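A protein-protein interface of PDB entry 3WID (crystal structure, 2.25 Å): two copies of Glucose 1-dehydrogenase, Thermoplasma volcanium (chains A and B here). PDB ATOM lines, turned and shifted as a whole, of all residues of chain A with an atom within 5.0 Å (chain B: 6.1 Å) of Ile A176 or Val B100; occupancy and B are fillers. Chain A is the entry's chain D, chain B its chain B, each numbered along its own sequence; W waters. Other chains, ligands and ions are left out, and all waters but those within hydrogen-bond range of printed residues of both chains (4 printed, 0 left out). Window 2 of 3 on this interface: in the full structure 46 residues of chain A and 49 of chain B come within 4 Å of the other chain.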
ATOM      1  N   ARG A 174      -1.338  26.546 -30.377  1.00  0.00           N
ATOM      2  CA  ARG A 174      -2.760  26.402 -30.680  1.00  0.00           C
ATOM      3  C   ARG A 174      -3.678  26.662 -29.461  1.00  0.00           C
ATOM      4  O   ARG A 174      -4.867  26.828 -29.601  1.00  0.00           O
ATOM      5  CB  ARG A 174      -3.088  25.073 -31.375  1.00  0.00           C
ATOM      6  CG  ARG A 174      -2.792  23.848 -30.595  1.00  0.00           C
ATOM      7  CD  ARG A 174      -2.977  22.580 -31.447  1.00  0.00           C
ATOM      8  NE  ARG A 174      -4.409  22.313 -31.542  1.00  0.00           N
ATOM      9  CZ  ARG A 174      -4.971  21.189 -31.882  1.00  0.00           C
ATOM     10  NH1 ARG A 174      -4.238  20.102 -32.218  1.00  0.00           N
ATOM     11  NH2 ARG A 174      -6.286  21.137 -31.863  1.00  0.00           N
ATOM     12  N   SER A 175      -3.124  26.673 -28.265  1.00  0.00           N
ATOM     13  CA  SER A 175      -3.925  26.893 -27.077  1.00  0.00           C
ATOM     14  C   SER A 175      -2.977  27.351 -25.988  1.00  0.00           C
ATOM     15  O   SER A 175      -1.782  27.521 -26.257  1.00  0.00           O
ATOM     16  CB  SER A 175      -4.579  25.633 -26.669  1.00  0.00           C
ATOM     17  OG  SER A 175      -3.575  24.721 -26.206  1.00  0.00           O
ATOM     18  N   ILE A 176      -3.472  27.617 -24.785  1.00  0.00           N
ATOM     19  CA  ILE A 176      -2.547  28.007 -23.707  1.00  0.00           C
ATOM     20  C   ILE A 176      -2.008  26.715 -23.099  1.00  0.00           C
ATOM     21  O   ILE A 176      -2.767  25.925 -22.513  1.00  0.00           O
ATOM     22  CB  ILE A 176      -3.206  28.866 -22.648  1.00  0.00           C
ATOM     23  CG1 ILE A 176      -3.562  30.208 -23.243  1.00  0.00           C
ATOM     24  CG2 ILE A 176      -2.238  29.062 -21.511  1.00  0.00           C
ATOM     25  CD1 ILE A 176      -4.378  31.053 -22.290  1.00  0.00           C
ATOM     26  N   PHE A 177      -0.717  26.472 -23.299  1.00  0.00           N
ATOM     27  CA  PHE A 177      -0.139  25.222 -22.852  1.00  0.00           C
ATOM     28  C   PHE A 177       0.290  25.391 -21.401  1.00  0.00           C
ATOM     29  O   PHE A 177       0.266  24.414 -20.662  1.00  0.00           O
ATOM     30  CB  PHE A 177       1.066  24.869 -23.709  1.00  0.00           C
ATOM     31  CG  PHE A 177       1.591  23.463 -23.520  1.00  0.00           C
ATOM     32  CD1 PHE A 177       1.091  22.420 -24.301  1.00  0.00           C
ATOM     33  CD2 PHE A 177       2.647  23.197 -22.631  1.00  0.00           C
ATOM     34  CE1 PHE A 177       1.597  21.130 -24.189  1.00  0.00           C
ATOM     35  CE2 PHE A 177       3.130  21.932 -22.498  1.00  0.00           C
ATOM     36  CZ  PHE A 177       2.637  20.891 -23.306  1.00  0.00           C
ATOM     37  N   GLN A 178       0.634  26.621 -21.005  1.00  0.00           N
ATOM     38  CA  GLN A 178       1.220  26.875 -19.675  1.00  0.00           C
ATOM     39  C   GLN A 178       0.166  26.836 -18.577  1.00  0.00           C
ATOM     40  O   GLN A 178      -1.055  26.829 -18.847  1.00  0.00           O
ATOM     41  CB  GLN A 178       1.925  28.205 -19.634  1.00  0.00           C
ATOM     42  CG  GLN A 178       3.012  28.388 -20.637  1.00  0.00           C
ATOM     43  CD  GLN A 178       2.490  28.659 -22.060  1.00  0.00           C
ATOM     44  OE1 GLN A 178       1.349  29.028 -22.272  1.00  0.00           O
ATOM     45  NE2 GLN A 178       3.334  28.479 -23.020  1.00  0.00           N
ATOM     46  N   ASN A 179       0.630  26.797 -17.330  1.00  0.00           N
ATOM     47  CA  ASN A 179      -0.280  26.906 -16.171  1.00  0.00           C
ATOM     48  C   ASN A 179      -0.790  28.345 -16.116  1.00  0.00           C
ATOM     49  O   ASN A 179      -0.247  29.232 -16.734  1.00  0.00           O
ATOM     50  CB  ASN A 179       0.435  26.624 -14.835  1.00  0.00           C
ATOM     51  CG  ASN A 179       1.035  25.208 -14.739  1.00  0.00           C
ATOM     52  OD1 ASN A 179       0.351  24.201 -14.832  1.00  0.00           O
ATOM     53  ND2 ASN A 179       2.329  25.161 -14.539  1.00  0.00           N
ATOM     54  N   ASP A 180      -1.822  28.558 -15.333  1.00  0.00           N
ATOM     55  CA  ASP A 180      -2.380  29.863 -15.157  1.00  0.00           C
ATOM     56  C   ASP A 180      -1.485  30.843 -14.409  1.00  0.00           C
ATOM     57  O   ASP A 180      -1.871  31.985 -14.257  1.00  0.00           O
ATOM     58  CB  ASP A 180      -3.747  29.804 -14.550  1.00  0.00           C
ATOM     59  CG  ASP A 180      -3.723  29.438 -13.097  1.00  0.00           C
ATOM     60  OD1 ASP A 180      -2.669  29.051 -12.618  1.00  0.00           O
ATOM     61  OD2 ASP A 180      -4.781  29.488 -12.463  1.00  0.00           O
ATOM     62  N   ASN A 269      -4.588  19.006 -24.930  1.00  0.00           N
ATOM     63  CA  ASN A 269      -3.600  19.931 -25.519  1.00  0.00           C
ATOM     64  C   ASN A 269      -2.172  19.415 -25.440  1.00  0.00           C
ATOM     65  O   ASN A 269      -1.244  20.172 -25.622  1.00  0.00           O
ATOM     66  CB  ASN A 269      -3.652  21.314 -24.862  1.00  0.00           C
ATOM     67  CG  ASN A 269      -5.060  21.881 -24.805  1.00  0.00           C
ATOM     68  OD1 ASN A 269      -5.883  21.695 -25.745  1.00  0.00           O
ATOM     69  ND2 ASN A 269      -5.331  22.626 -23.752  1.00  0.00           N
ATOM     70  N   LYS B  98     -13.287  26.314 -15.501  1.00  0.00           N
ATOM     71  CA  LYS B  98     -12.393  27.252 -14.763  1.00  0.00           C
ATOM     72  C   LYS B  98     -10.912  27.249 -15.161  1.00  0.00           C
ATOM     73  O   LYS B  98     -10.165  28.126 -14.704  1.00  0.00           O
ATOM     74  CB  LYS B  98     -12.473  26.878 -13.260  1.00  0.00           C
ATOM     75  CG  LYS B  98     -13.688  27.465 -12.558  1.00  0.00           C
ATOM     76  CD  LYS B  98     -15.026  26.852 -12.924  1.00  0.00           C
ATOM     77  CE  LYS B  98     -16.192  27.541 -12.159  1.00  0.00           C
ATOM     78  NZ  LYS B  98     -16.144  27.161 -10.709  1.00  0.00           N
ATOM     79  N   CYS B  99     -10.485  26.264 -15.964  1.00  0.00           N
ATOM     80  CA  CYS B  99      -9.088  26.114 -16.358  1.00  0.00           C
ATOM     81  C   CYS B  99      -8.644  27.326 -17.161  1.00  0.00           C
ATOM     82  O   CYS B  99      -9.420  28.176 -17.485  1.00  0.00           O
ATOM     83  CB  CYS B  99      -8.874  24.847 -17.195  1.00  0.00           C
ATOM     84  SG  CYS B  99      -9.524  24.893 -18.917  1.00  0.00           S
ATOM     85  N   VAL B 100      -7.366  27.395 -17.415  1.00  0.00           N
ATOM     86  CA  VAL B 100      -6.746  28.546 -17.981  1.00  0.00           C
ATOM     87  C   VAL B 100      -7.297  28.871 -19.414  1.00  0.00           C
ATOM     88  O   VAL B 100      -7.301  30.049 -19.809  1.00  0.00           O
ATOM     89  CB  VAL B 100      -5.202  28.365 -17.957  1.00  0.00           C
ATOM     90  CG1 VAL B 100      -4.728  27.219 -18.872  1.00  0.00           C
ATOM     91  CG2 VAL B 100      -4.522  29.651 -18.296  1.00  0.00           C
ATOM     92  N   ASN B 101      -7.735  27.841 -20.147  1.00  0.00           N
ATOM     93  CA  ASN B 101      -8.376  28.028 -21.447  1.00  0.00           C
ATOM     94  C   ASN B 101      -9.865  28.428 -21.434  1.00  0.00           C
ATOM     95  O   ASN B 101     -10.232  29.299 -22.175  1.00  0.00           O
ATOM     96  CB  ASN B 101      -8.176  26.799 -22.333  1.00  0.00           C
ATOM     97  CG  ASN B 101      -6.730  26.681 -22.818  1.00  0.00           C
ATOM     98  OD1 ASN B 101      -6.297  27.416 -23.739  1.00  0.00           O
ATOM     99  ND2 ASN B 101      -5.976  25.786 -22.179  1.00  0.00           N
ATOM    100  N   CYS B 102     -10.684  27.754 -20.627  1.00  0.00           N
ATOM    101  CA  CYS B 102     -12.060  28.119 -20.375  1.00  0.00           C
ATOM    102  C   CYS B 102     -12.300  29.574 -19.924  1.00  0.00           C
ATOM    103  O   CYS B 102     -13.208  30.251 -20.382  1.00  0.00           O
ATOM    104  CB  CYS B 102     -12.659  27.138 -19.351  1.00  0.00           C
ATOM    105  SG  CYS B 102     -13.027  25.484 -20.028  1.00  0.00           S
ATOM    106  N   ARG B 103     -11.438  30.091 -19.072  1.00  0.00           N
ATOM    107  CA  ARG B 103     -11.686  31.363 -18.497  1.00  0.00           C
ATOM    108  C   ARG B 103     -11.420  32.514 -19.419  1.00  0.00           C
ATOM    109  O   ARG B 103     -11.754  33.673 -19.077  1.00  0.00           O
ATOM    110  CB  ARG B 103     -10.947  31.474 -17.165  1.00  0.00           C
ATOM    111  CG  ARG B 103      -9.436  31.617 -17.188  1.00  0.00           C
ATOM    112  CD  ARG B 103      -9.028  30.701 -16.081  1.00  0.00           C
ATOM    113  NE  ARG B 103      -8.014  31.202 -15.283  1.00  0.00           N
ATOM    114  CZ  ARG B 103      -7.393  30.475 -14.333  1.00  0.00           C
ATOM    115  NH1 ARG B 103      -7.626  29.198 -14.137  1.00  0.00           N
ATOM    116  NH2 ARG B 103      -6.498  31.064 -13.625  1.00  0.00           N
ATOM    117  N   ILE B 104     -10.798  32.231 -20.578  1.00  0.00           N
ATOM    118  CA  ILE B 104     -10.566  33.263 -21.586  1.00  0.00           C
ATOM    119  C   ILE B 104     -11.469  33.082 -22.784  1.00  0.00           C
ATOM    120  O   ILE B 104     -11.241  33.705 -23.856  1.00  0.00           O
ATOM    121  CB  ILE B 104      -9.090  33.352 -22.001  1.00  0.00           C
ATOM    122  CG1 ILE B 104      -8.599  32.092 -22.733  1.00  0.00           C
ATOM    123  CG2 ILE B 104      -8.259  33.600 -20.769  1.00  0.00           C
ATOM    124  CD1 ILE B 104      -7.570  32.361 -23.817  1.00  0.00           C
ATOM    125  N   ASN B 109     -10.625  24.601 -26.076  1.00  0.00           N
ATOM    126  CA  ASN B 109      -9.339  23.990 -25.746  1.00  0.00           C
ATOM    127  C   ASN B 109      -9.157  23.705 -24.249  1.00  0.00           C
ATOM    128  O   ASN B 109      -8.043  23.797 -23.751  1.00  0.00           O
ATOM    129  CB  ASN B 109      -8.205  24.902 -26.196  1.00  0.00           C
ATOM    130  CG  ASN B 109      -8.186  25.071 -27.681  1.00  0.00           C
ATOM    131  OD1 ASN B 109      -8.511  24.118 -28.409  1.00  0.00           O
ATOM    132  ND2 ASN B 109      -7.839  26.246 -28.137  1.00  0.00           N
ATOM    133  N   SER B 111      -8.188  22.506 -20.914  1.00  0.00           N
ATOM    134  CA  SER B 111      -7.086  21.701 -20.434  1.00  0.00           C
ATOM    135  C   SER B 111      -7.529  20.509 -19.568  1.00  0.00           C
ATOM    136  O   SER B 111      -6.708  19.701 -19.211  1.00  0.00           O
ATOM    137  CB  SER B 111      -6.199  22.538 -19.588  1.00  0.00           C
ATOM    138  OG  SER B 111      -5.823  23.690 -20.267  1.00  0.00           O
HETATM  139  O   HOH W   1      -6.977  26.489 -31.168  1.00  0.00           O
HETATM  140  O   HOH W   2      -8.181  20.758 -25.075  1.00  0.00           O
HETATM  141  O   HOH W   3      -3.359  23.397 -21.462  1.00  0.00           O
HETATM  142  O   HOH W   4      -6.601  23.887 -30.589  1.00  0.00           O
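N of Ile A176 is in hydrogen-bond range of OD1 of Asn B101, 3.0 Å away. The guanidinium group (NH2) of Arg B103 is in salt-bridge range of the side-chain carboxylate (OD2) of Asp A180 (2.6 Å). O of Arg A174 sits at hydrogen-bond distance from ND2 of Asn B109 (3.4 Å). The backbone carbonyl oxygen (O) of Asn B109 lies within hydrogen-bond range of the side-chain amide nitrogen (ND2) of Asn A269, 3.0 Å away.
O of Lys B98 lies within hydrogen-bond range of NH1 of Arg B103 (2.8 Å). The side-chain sulfur (SG) of Cys B99 lies close to the backbone NH (N) of Asn B101, 3.7 Å away. The side-chain sulfur (SG) of Cys B99 lies close to the backbone NH (N) of Ser B111, at 3.4 Å. The side-chain amide nitrogen of Asn B101 lies within hydrogen-bond range of the backbone carbonyl oxygen of Asn B109 (3.3 Å). The side-chain hydroxyl (OG) of Ser B111 sits at hydrogen-bond distance from the side-chain amide nitrogen (ND2) of Asn B101, at 2.8 Å.
Among the printed residues, pairs that only touch across the chains: Ser A175 with Asn B101 (3.8 Å), Ser A175 with Asn B109 (3.6 Å), Ile A176 with Val B100 (3.96 Å), Ile A176 with Ile B104 (3.8 Å), Gln A178 with Val B100 (3.7 Å), Asp A180 with Val B100 (3.8 Å), Asn A269 with Asn B101 (3.6 Å) and Asn A269 with Ser B111 (3.7 Å).
Of chain B, only Val B100, Asn B101 and Ile B104 come within 4 Å of Ile A176. Val B100 touches three residues of chain A. Printed residues of chain B within 4 Å of Asp A180: Val B100 (3.8 Å) and Arg B103 (2.6 Å). Printed residues of chain A within 4 Å of Asn B101: Ser A175, Ile A176 and Asn A269. Of the printed residues of chain A, Ser B111 touches Asn A269 (3.7 Å). Printed residues of chain B within 4 Å of Gln A178: Val B100. Of the printed residues of chain B, Asn A269 touches Asn B101, Asn B109 and Ser B111. Cys B102 touches none of the printed residues of chain A. The nearest residue of chain B that does not touch Ile A176 is Ser B111 (4.4 Å). The nearest printed residue of chain A that does not touch Ser B111 is Ile A176 (4.4 Å).
Of the 9 printed residues of chain B, 6 touch a printed residue of chain A.
No position is printed for both chains.
Water W2 bridges OD1 of Asn A269 (2.6 Å) and O of Asn B109 (3.3 Å). Water W1 lies within hydrogen-bond range of the backbone carbonyl oxygen (O) of Arg A174 (2.7 Å) and the side-chain amide nitrogen (ND2) of Asn B109 (3.2 Å). Water W3 lies within hydrogen-bond range of the side-chain hydroxyl of Ser B111 (2.8 Å), the backbone carbonyl oxygen of Ile A176 (2.8 Å) and the side-chain amide nitrogen of Asn A269 (3.1 Å). Water W4 lies within hydrogen-bond range of the guanidinium group of Arg A174 and the side-chain amide oxygen of Asn B109.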
